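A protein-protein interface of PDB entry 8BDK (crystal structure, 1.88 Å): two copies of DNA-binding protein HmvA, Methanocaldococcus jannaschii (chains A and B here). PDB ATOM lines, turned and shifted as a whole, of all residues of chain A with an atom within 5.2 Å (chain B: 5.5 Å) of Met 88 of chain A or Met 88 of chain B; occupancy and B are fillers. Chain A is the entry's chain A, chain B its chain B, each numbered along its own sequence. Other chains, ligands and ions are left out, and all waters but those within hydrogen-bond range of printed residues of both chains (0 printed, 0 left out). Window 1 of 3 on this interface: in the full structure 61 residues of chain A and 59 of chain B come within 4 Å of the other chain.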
ATOM      1  N   MET A  30      -7.256  11.949  -3.792  1.00  0.00           N
ATOM      2  CA  MET A  30      -7.168  10.820  -2.869  1.00  0.00           C
ATOM      3  C   MET A  30      -6.105   9.830  -3.311  1.00  0.00           C
ATOM      4  O   MET A  30      -5.335   9.330  -2.483  1.00  0.00           O
ATOM      5  CB  MET A  30      -8.510  10.098  -2.759  1.00  0.00           C
ATOM      6  CG  MET A  30      -9.636  10.908  -2.171  1.00  0.00           C
ATOM      7  SD  MET A  30     -11.220  10.132  -2.616  1.00  0.00           S
ATOM      8  CE  MET A  30     -10.975   8.443  -2.009  1.00  0.00           C
ATOM      9  N   ILE A  34      -2.832   8.532  -1.289  1.00  0.00           N
ATOM     10  CA  ILE A  34      -2.574   7.112  -1.047  1.00  0.00           C
ATOM     11  C   ILE A  34      -1.161   6.741  -1.471  1.00  0.00           C
ATOM     12  O   ILE A  34      -0.440   6.044  -0.738  1.00  0.00           O
ATOM     13  CB  ILE A  34      -3.616   6.250  -1.777  1.00  0.00           C
ATOM     14  CG1 ILE A  34      -4.926   6.264  -1.001  1.00  0.00           C
ATOM     15  CG2 ILE A  34      -3.108   4.818  -1.952  1.00  0.00           C
ATOM     16  CD1 ILE A  34      -6.130   6.321  -1.879  1.00  0.00           C
ATOM     17  N   THR A  38       1.458   5.308   1.327  1.00  0.00           N
ATOM     18  CA  THR A  38       1.941   3.937   1.130  1.00  0.00           C
ATOM     19  C   THR A  38       3.451   3.932   0.942  1.00  0.00           C
ATOM     20  O   THR A  38       4.167   3.105   1.527  1.00  0.00           O
ATOM     21  CB  THR A  38       1.280   3.263  -0.078  1.00  0.00           C
ATOM     22  OG1 THR A  38      -0.151   3.261   0.039  1.00  0.00           O
ATOM     23  CG2 THR A  38       1.777   1.776  -0.187  1.00  0.00           C
ATOM     24  N   ILE A  83      -8.558  15.431   5.331  1.00  0.00           N
ATOM     25  CA  ILE A  83      -9.837  15.266   4.640  1.00  0.00           C
ATOM     26  C   ILE A  83      -9.763  14.124   3.643  1.00  0.00           C
ATOM     27  O   ILE A  83     -10.690  13.316   3.526  1.00  0.00           O
ATOM     28  CB  ILE A  83     -10.255  16.568   3.934  1.00  0.00           C
ATOM     29  CG1 ILE A  83     -10.617  17.651   4.948  1.00  0.00           C
ATOM     30  CG2 ILE A  83     -11.426  16.287   2.999  1.00  0.00           C
ATOM     31  CD1 ILE A  83     -11.534  17.175   6.025  1.00  0.00           C
ATOM     32  N   LEU A  84      -8.664  14.053   2.894  1.00  0.00           N
ATOM     33  CA  LEU A  84      -8.509  12.986   1.915  1.00  0.00           C
ATOM     34  C   LEU A  84      -8.545  11.610   2.567  1.00  0.00           C
ATOM     35  O   LEU A  84      -9.036  10.653   1.959  1.00  0.00           O
ATOM     36  CB  LEU A  84      -7.208  13.186   1.137  1.00  0.00           C
ATOM     37  CG  LEU A  84      -7.207  14.389   0.194  1.00  0.00           C
ATOM     38  CD1 LEU A  84      -5.785  14.771  -0.249  1.00  0.00           C
ATOM     39  CD2 LEU A  84      -8.112  14.152  -1.013  1.00  0.00           C
ATOM     40  N   ILE A  85      -8.037  11.489   3.794  1.00  0.00           N
ATOM     41  CA  ILE A  85      -8.078  10.208   4.494  1.00  0.00           C
ATOM     42  C   ILE A  85      -9.481   9.920   5.013  1.00  0.00           C
ATOM     43  O   ILE A  85      -9.946   8.785   4.945  1.00  0.00           O
ATOM     44  CB  ILE A  85      -7.043  10.176   5.634  1.00  0.00           C
ATOM     45  CG1 ILE A  85      -5.617  10.221   5.074  1.00  0.00           C
ATOM     46  CG2 ILE A  85      -7.255   8.937   6.507  1.00  0.00           C
ATOM     47  CD1 ILE A  85      -5.242   9.004   4.253  1.00  0.00           C
ATOM     48  N   LYS A  86     -10.172  10.932   5.564  1.00  0.00           N
ATOM     49  CA  LYS A  86     -11.563  10.736   5.959  1.00  0.00           C
ATOM     50  C   LYS A  86     -12.393  10.248   4.777  1.00  0.00           C
ATOM     51  O   LYS A  86     -13.267   9.387   4.933  1.00  0.00           O
ATOM     52  CB  LYS A  86     -12.172  12.037   6.498  1.00  0.00           C
ATOM     53  CG  LYS A  86     -11.573  12.599   7.790  1.00  0.00           C
ATOM     54  CD  LYS A  86     -12.379  13.829   8.258  1.00  0.00           C
ATOM     55  CE  LYS A  86     -11.742  14.544   9.449  1.00  0.00           C
ATOM     56  NZ  LYS A  86     -12.659  15.569  10.045  1.00  0.00           N
ATOM     57  N   GLU A  87     -12.146  10.810   3.590  1.00  0.00           N
ATOM     58  CA  GLU A  87     -12.893  10.414   2.403  1.00  0.00           C
ATOM     59  C   GLU A  87     -12.619   8.961   2.051  1.00  0.00           C
ATOM     60  O   GLU A  87     -13.544   8.198   1.747  1.00  0.00           O
ATOM     61  CB  GLU A  87     -12.549  11.337   1.234  1.00  0.00           C
ATOM     62  CG  GLU A  87     -13.327  12.650   1.290  1.00  0.00           C
ATOM     63  CD  GLU A  87     -12.841  13.680   0.304  1.00  0.00           C
ATOM     64  OE1 GLU A  87     -11.943  13.372  -0.505  1.00  0.00           O
ATOM     65  OE2 GLU A  87     -13.369  14.809   0.335  1.00  0.00           O
ATOM     66  N   MET A  88     -11.342   8.562   2.066  1.00  0.00           N
ATOM     67  CA  MET A  88     -10.992   7.164   1.847  1.00  0.00           C
ATOM     68  C   MET A  88     -11.730   6.258   2.828  1.00  0.00           C
ATOM     69  O   MET A  88     -12.331   5.249   2.436  1.00  0.00           O
ATOM     70  CB  MET A  88      -9.477   6.994   1.992  1.00  0.00           C
ATOM     71  CG  MET A  88      -8.731   7.079   0.682  1.00  0.00           C
ATOM     72  SD  MET A  88      -9.130   5.643  -0.321  1.00  0.00           S
ATOM     73  CE  MET A  88      -8.719   4.341   0.807  1.00  0.00           C
ATOM     74  N   LEU A  89     -11.680   6.607   4.109  1.00  0.00           N
ATOM     75  CA  LEU A  89     -12.314   5.777   5.129  1.00  0.00           C
ATOM     76  C   LEU A  89     -13.822   5.773   4.963  1.00  0.00           C
ATOM     77  O   LEU A  89     -14.480   4.757   5.212  1.00  0.00           O
ATOM     78  CB  LEU A  89     -11.930   6.276   6.521  1.00  0.00           C
ATOM     79  CG  LEU A  89     -10.471   5.999   6.889  1.00  0.00           C
ATOM     80  CD1 LEU A  89     -10.127   6.528   8.276  1.00  0.00           C
ATOM     81  CD2 LEU A  89     -10.222   4.501   6.819  1.00  0.00           C
ATOM     82  N   ASN A  90     -14.386   6.911   4.563  1.00  0.00           N
ATOM     83  CA  ASN A  90     -15.819   6.969   4.291  1.00  0.00           C
ATOM     84  C   ASN A  90     -16.197   5.983   3.197  1.00  0.00           C
ATOM     85  O   ASN A  90     -17.190   5.255   3.319  1.00  0.00           O
ATOM     86  CB  ASN A  90     -16.211   8.391   3.900  1.00  0.00           C
ATOM     87  CG  ASN A  90     -17.682   8.653   4.075  1.00  0.00           C
ATOM     88  OD1 ASN A  90     -18.477   8.409   3.168  1.00  0.00           O
ATOM     89  ND2 ASN A  90     -18.059   9.154   5.247  1.00  0.00           N
ATOM     90  N   VAL A  91     -15.397   5.936   2.129  1.00  0.00           N
ATOM     91  CA  VAL A  91     -15.623   4.989   1.037  1.00  0.00           C
ATOM     92  C   VAL A  91     -15.517   3.555   1.546  1.00  0.00           C
ATOM     93  O   VAL A  91     -16.397   2.718   1.296  1.00  0.00           O
ATOM     94  CB  VAL A  91     -14.617   5.246  -0.098  1.00  0.00           C
ATOM     95  CG1 VAL A  91     -14.657   4.115  -1.102  1.00  0.00           C
ATOM     96  CG2 VAL A  91     -14.870   6.576  -0.775  1.00  0.00           C
ATOM     97  N   ILE A  92     -14.426   3.251   2.269  1.00  0.00           N
ATOM     98  CA  ILE A  92     -14.194   1.888   2.740  1.00  0.00           C
ATOM     99  C   ILE A  92     -15.308   1.448   3.675  1.00  0.00           C
ATOM    100  O   ILE A  92     -15.780   0.308   3.605  1.00  0.00           O
ATOM    101  CB  ILE A  92     -12.815   1.774   3.422  1.00  0.00           C
ATOM    102  CG1 ILE A  92     -11.696   2.103   2.431  1.00  0.00           C
ATOM    103  CG2 ILE A  92     -12.617   0.362   3.995  1.00  0.00           C
ATOM    104  CD1 ILE A  92     -10.308   2.162   3.062  1.00  0.00           C
ATOM    105  N   THR A  93     -15.747   2.332   4.571  1.00  0.00           N
ATOM    106  CA  THR A  93     -16.799   1.930   5.497  1.00  0.00           C
ATOM    107  C   THR A  93     -18.158   1.878   4.813  1.00  0.00           C
ATOM    108  O   THR A  93     -18.993   1.041   5.176  1.00  0.00           O
ATOM    109  CB  THR A  93     -16.827   2.854   6.718  1.00  0.00           C
ATOM    110  OG1 THR A  93     -16.974   4.219   6.306  1.00  0.00           O
ATOM    111  CG2 THR A  93     -15.541   2.714   7.501  1.00  0.00           C
ATOM    112  N   MET B  30      -3.632  -1.681  -5.421  1.00  0.00           N
ATOM    113  CA  MET B  30      -4.356  -0.918  -4.410  1.00  0.00           C
ATOM    114  C   MET B  30      -5.070   0.256  -5.031  1.00  0.00           C
ATOM    115  O   MET B  30      -6.231   0.516  -4.716  1.00  0.00           O
ATOM    116  CB  MET B  30      -3.404  -0.417  -3.320  1.00  0.00           C
ATOM    117  CG  MET B  30      -2.803  -1.528  -2.481  1.00  0.00           C
ATOM    118  SD  MET B  30      -1.518  -0.927  -1.361  1.00  0.00           S
ATOM    119  CE  MET B  30      -2.469   0.235  -0.393  1.00  0.00           C
ATOM    120  N   ILE B  34      -9.045   1.118  -5.105  1.00  0.00           N
ATOM    121  CA  ILE B  34      -9.601   2.382  -4.602  1.00  0.00           C
ATOM    122  C   ILE B  34     -10.463   3.057  -5.659  1.00  0.00           C
ATOM    123  O   ILE B  34     -11.533   3.600  -5.350  1.00  0.00           O
ATOM    124  CB  ILE B  34      -8.475   3.312  -4.121  1.00  0.00           C
ATOM    125  CG1 ILE B  34      -7.875   2.766  -2.857  1.00  0.00           C
ATOM    126  CG2 ILE B  34      -9.012   4.738  -3.835  1.00  0.00           C
ATOM    127  CD1 ILE B  34      -6.414   3.017  -2.791  1.00  0.00           C
ATOM    128  N   THR B  38     -14.386   3.636  -4.682  1.00  0.00           N
ATOM    129  CA  THR B  38     -14.778   5.046  -4.625  1.00  0.00           C
ATOM    130  C   THR B  38     -15.871   5.339  -5.646  1.00  0.00           C
ATOM    131  O   THR B  38     -16.851   6.027  -5.339  1.00  0.00           O
ATOM    132  CB  THR B  38     -13.561   5.949  -4.856  1.00  0.00           C
ATOM    133  OG1 THR B  38     -12.559   5.738  -3.832  1.00  0.00           O
ATOM    134  CG2 THR B  38     -13.963   7.430  -4.820  1.00  0.00           C
ATOM    135  N   ILE B  83      -7.776  -8.469   0.703  1.00  0.00           N
ATOM    136  CA  ILE B  83      -6.388  -8.179   1.070  1.00  0.00           C
ATOM    137  C   ILE B  83      -6.025  -6.735   0.740  1.00  0.00           C
ATOM    138  O   ILE B  83      -5.351  -6.049   1.525  1.00  0.00           O
ATOM    139  CB  ILE B  83      -5.442  -9.182   0.382  1.00  0.00           C
ATOM    140  CG1 ILE B  83      -5.708 -10.600   0.903  1.00  0.00           C
ATOM    141  CG2 ILE B  83      -3.987  -8.815   0.612  1.00  0.00           C
ATOM    142  CD1 ILE B  83      -4.971 -11.695   0.138  1.00  0.00           C
ATOM    143  N   LEU B  84      -6.488  -6.239  -0.412  1.00  0.00           N
ATOM    144  CA  LEU B  84      -6.113  -4.890  -0.837  1.00  0.00           C
ATOM    145  C   LEU B  84      -6.673  -3.829   0.104  1.00  0.00           C
ATOM    146  O   LEU B  84      -6.019  -2.809   0.351  1.00  0.00           O
ATOM    147  CB  LEU B  84      -6.592  -4.637  -2.265  1.00  0.00           C
ATOM    148  CG  LEU B  84      -5.794  -5.332  -3.365  1.00  0.00           C
ATOM    149  CD1 LEU B  84      -6.447  -5.111  -4.714  1.00  0.00           C
ATOM    150  CD2 LEU B  84      -4.355  -4.845  -3.376  1.00  0.00           C
ATOM    151  N   ILE B  85      -7.887  -4.045   0.619  1.00  0.00           N
ATOM    152  CA  ILE B  85      -8.463  -3.141   1.606  1.00  0.00           C
ATOM    153  C   ILE B  85      -7.691  -3.223   2.922  1.00  0.00           C
ATOM    154  O   ILE B  85      -7.497  -2.212   3.612  1.00  0.00           O
ATOM    155  CB  ILE B  85      -9.951  -3.465   1.811  1.00  0.00           C
ATOM    156  CG1 ILE B  85     -10.738  -3.251   0.512  1.00  0.00           C
ATOM    157  CG2 ILE B  85     -10.519  -2.654   2.962  1.00  0.00           C
ATOM    158  CD1 ILE B  85     -10.557  -1.903  -0.104  1.00  0.00           C
ATOM    159  N   LYS B  86      -7.289  -4.427   3.313  1.00  0.00           N
ATOM    160  CA  LYS B  86      -6.467  -4.589   4.512  1.00  0.00           C
ATOM    161  C   LYS B  86      -5.146  -3.841   4.380  1.00  0.00           C
ATOM    162  O   LYS B  86      -4.667  -3.228   5.345  1.00  0.00           O
ATOM    163  CB  LYS B  86      -6.196  -6.077   4.770  1.00  0.00           C
ATOM    164  CG  LYS B  86      -7.369  -6.880   5.321  1.00  0.00           C
ATOM    165  CD  LYS B  86      -6.983  -8.355   5.520  1.00  0.00           C
ATOM    166  CE  LYS B  86      -5.766  -8.490   6.426  1.00  0.00           C
ATOM    167  NZ  LYS B  86      -5.304  -9.906   6.586  1.00  0.00           N
ATOM    168  N   GLU B  87      -4.526  -3.900   3.206  1.00  0.00           N
ATOM    169  CA  GLU B  87      -3.261  -3.196   3.032  1.00  0.00           C
ATOM    170  C   GLU B  87      -3.468  -1.693   3.074  1.00  0.00           C
ATOM    171  O   GLU B  87      -2.648  -0.967   3.645  1.00  0.00           O
ATOM    172  CB  GLU B  87      -2.597  -3.609   1.726  1.00  0.00           C
ATOM    173  CG  GLU B  87      -2.091  -5.036   1.743  1.00  0.00           C
ATOM    174  CD  GLU B  87      -1.558  -5.480   0.399  1.00  0.00           C
ATOM    175  OE1 GLU B  87      -1.864  -4.823  -0.616  1.00  0.00           O
ATOM    176  OE2 GLU B  87      -0.829  -6.481   0.356  1.00  0.00           O
ATOM    177  N   MET B  88      -4.547  -1.205   2.461  1.00  0.00           N
ATOM    178  CA  MET B  88      -4.859   0.214   2.565  1.00  0.00           C
ATOM    179  C   MET B  88      -5.026   0.633   4.022  1.00  0.00           C
ATOM    180  O   MET B  88      -4.433   1.627   4.467  1.00  0.00           O
ATOM    181  CB  MET B  88      -6.114   0.525   1.755  1.00  0.00           C
ATOM    182  CG  MET B  88      -6.682   1.899   2.037  1.00  0.00           C
ATOM    183  SD  MET B  88      -5.486   3.209   1.765  1.00  0.00           S
ATOM    184  CE  MET B  88      -4.824   2.738   0.190  1.00  0.00           C
ATOM    185  N   LEU B  89      -5.838  -0.106   4.778  1.00  0.00           N
ATOM    186  CA  LEU B  89      -6.066   0.207   6.179  1.00  0.00           C
ATOM    187  C   LEU B  89      -4.802   0.044   7.007  1.00  0.00           C
ATOM    188  O   LEU B  89      -4.599   0.792   7.966  1.00  0.00           O
ATOM    189  CB  LEU B  89      -7.187  -0.669   6.740  1.00  0.00           C
ATOM    190  CG  LEU B  89      -8.560  -0.340   6.152  1.00  0.00           C
ATOM    191  CD1 LEU B  89      -9.564  -1.380   6.596  1.00  0.00           C
ATOM    192  CD2 LEU B  89      -8.994   1.075   6.577  1.00  0.00           C
ATOM    193  N   ASN B  90      -3.944  -0.918   6.665  1.00  0.00           N
ATOM    194  CA  ASN B  90      -2.681  -1.024   7.385  1.00  0.00           C
ATOM    195  C   ASN B  90      -1.819   0.204   7.139  1.00  0.00           C
ATOM    196  O   ASN B  90      -1.196   0.732   8.064  1.00  0.00           O
ATOM    197  CB  ASN B  90      -1.928  -2.288   6.980  1.00  0.00           C
ATOM    198  CG  ASN B  90      -0.761  -2.590   7.920  1.00  0.00           C
ATOM    199  OD1 ASN B  90      -0.927  -2.633   9.138  1.00  0.00           O
ATOM    200  ND2 ASN B  90       0.426  -2.778   7.356  1.00  0.00           N
ATOM    201  N   VAL B  91      -1.778   0.670   5.891  1.00  0.00           N
ATOM    202  CA  VAL B  91      -1.048   1.887   5.561  1.00  0.00           C
ATOM    203  C   VAL B  91      -1.616   3.078   6.336  1.00  0.00           C
ATOM    204  O   VAL B  91      -0.877   3.828   6.989  1.00  0.00           O
ATOM    205  CB  VAL B  91      -1.073   2.117   4.037  1.00  0.00           C
ATOM    206  CG1 VAL B  91      -0.730   3.562   3.699  1.00  0.00           C
ATOM    207  CG2 VAL B  91      -0.109   1.149   3.348  1.00  0.00           C
ATOM    208  N   ILE B  92      -2.942   3.243   6.317  1.00  0.00           N
ATOM    209  CA  ILE B  92      -3.560   4.398   6.972  1.00  0.00           C
ATOM    210  C   ILE B  92      -3.312   4.390   8.477  1.00  0.00           C
ATOM    211  O   ILE B  92      -3.116   5.449   9.091  1.00  0.00           O
ATOM    212  CB  ILE B  92      -5.068   4.448   6.646  1.00  0.00           C
ATOM    213  CG1 ILE B  92      -5.269   4.722   5.146  1.00  0.00           C
ATOM    214  CG2 ILE B  92      -5.751   5.502   7.492  1.00  0.00           C
ATOM    215  CD1 ILE B  92      -6.735   4.698   4.681  1.00  0.00           C
ATOM    216  N   THR B  93      -3.362   3.208   9.106  1.00  0.00           N
ATOM    217  CA  THR B  93      -3.123   3.109  10.544  1.00  0.00           C
ATOM    218  C   THR B  93      -1.644   3.054  10.905  1.00  0.00           C
ATOM    219  O   THR B  93      -1.312   3.173  12.086  1.00  0.00           O
ATOM    220  CB  THR B  93      -3.805   1.874  11.147  1.00  0.00           C
ATOM    221  OG1 THR B  93      -3.266   0.691  10.548  1.00  0.00           O
ATOM    222  CG2 THR B  93      -5.312   1.922  10.937  1.00  0.00           C
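Of the 14 printed residues of chain A, 8 touch a printed residue of chain B.
Hydrophobic or aromatic side chains of chain A within 4 Å of the printed part of chain B: Met 30, Ile 34, Ile 85, Met 88, Leu 89, Val 91 and Ile 92.
Hydrophobic or aromatic side chains of chain B within 4 Å of the printed part of chain A: Met 30, Ile 34, Ile 85, Met 88, Leu 89, Val 91 and Ile 92.
Among the printed residues, 13 pairs touch across the chains.
Among the printed residues, no Asp or Glu carboxylate lies within 4 Å of a Lys or Arg side-chain nitrogen of the other chain.
Ile 34 of chain A touches its own counterpart, Ile 34 of chain B.
Ile 34 of chain A touches Met 88 of chain B, and with the chains exchanged Met 88 of chain A touches Ile 34 of chain B.
Thr 38 of chain A touches Val 91 of chain B, and with the chains exchanged Val 91 of chain A touches Thr 38 of chain B.
Ile 92 of chain A touches Met 88 of chain B, but with the chains exchanged Met 88 of chain A does not touch Ile 92 of chain B (4.4 Å).
14 positions are printed for both chains.
Of the 13 pairs that touch across the chains among the printed residues, 11 have their exchanged pair printed and touching as well.
Among the printed residues, merely in contact across the chains: Met 88 of chain A with Met 88 of chain B, Ile 34 of chain A with Ile 34 of chain B, Ile 34 of chain A with Met 88 of chain B, Val 91 of chain A with Thr 38 of chain B, Met 30 of chain A with Thr 38 of chain B, Met 88 of chain A with Ile 34 of chain B, Leu 89 of chain A with Leu 89 of chain B, Thr 38 of chain A with Val 91 of chain B, Ile 92 of chain A with Met 88 of chain B, Ile 92 of chain A with Ile 85 of chain B, Thr 38 of chain A with Met 30 of chain B, Ile 85 of chain A with Ile 92 of chain B and Ile 92 of chain A with Leu 89 of chain B.
O of Ile 34 of chain A sits at hydrogen-bond distance from OG1 of Thr 38 of chain A (2.9 Å).
The backbone carbonyl oxygen (O) of Leu 89 of chain A is in hydrogen-bond range of the side-chain hydroxyl (OG1) of Thr 93 of chain A, at 2.8 Å.
The backbone carbonyl oxygen (O) of Ile 34 of chain B sits at hydrogen-bond distance from the side-chain hydroxyl (OG1) of Thr 38 of chain B (2.8 Å).
The backbone carbonyl oxygen (O) of Leu 89 of chain B lies within hydrogen-bond range of the side-chain hydroxyl (OG1) of Thr 93 of chain B (2.9 Å).
Of the printed residues of chain B, Met 88 of chain A touches Ile 34 and Met 88.
Of the printed residues of chain A, Met 88 of chain B touches Ile 34, Met 88 and Ile 92.
Printed residues of chain B within 4 Å of Ile 85 of chain A: Ile 92.
Of the printed residues of chain B, Ile 34 of chain A touches Ile 34 (3.4 Å) and Met 88 (3.4 Å).
Of the printed residues of chain B, Leu 89 of chain A touches Leu 89.
Of the printed residues of chain A, Val 91 of chain B touches Thr 38.
Ile 83 of chain B touches none of the printed residues of chain A.
Ile 83 of chain A touches none of the printed residues of chain B.
The nearest printed residue of chain B that does not touch Met 88 of chain A is Ile 92 of chain B (4.4 Å).
The nearest printed residue of chain A that does not touch Met 88 of chain B is Thr 38 of chain A (4.7 Å).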
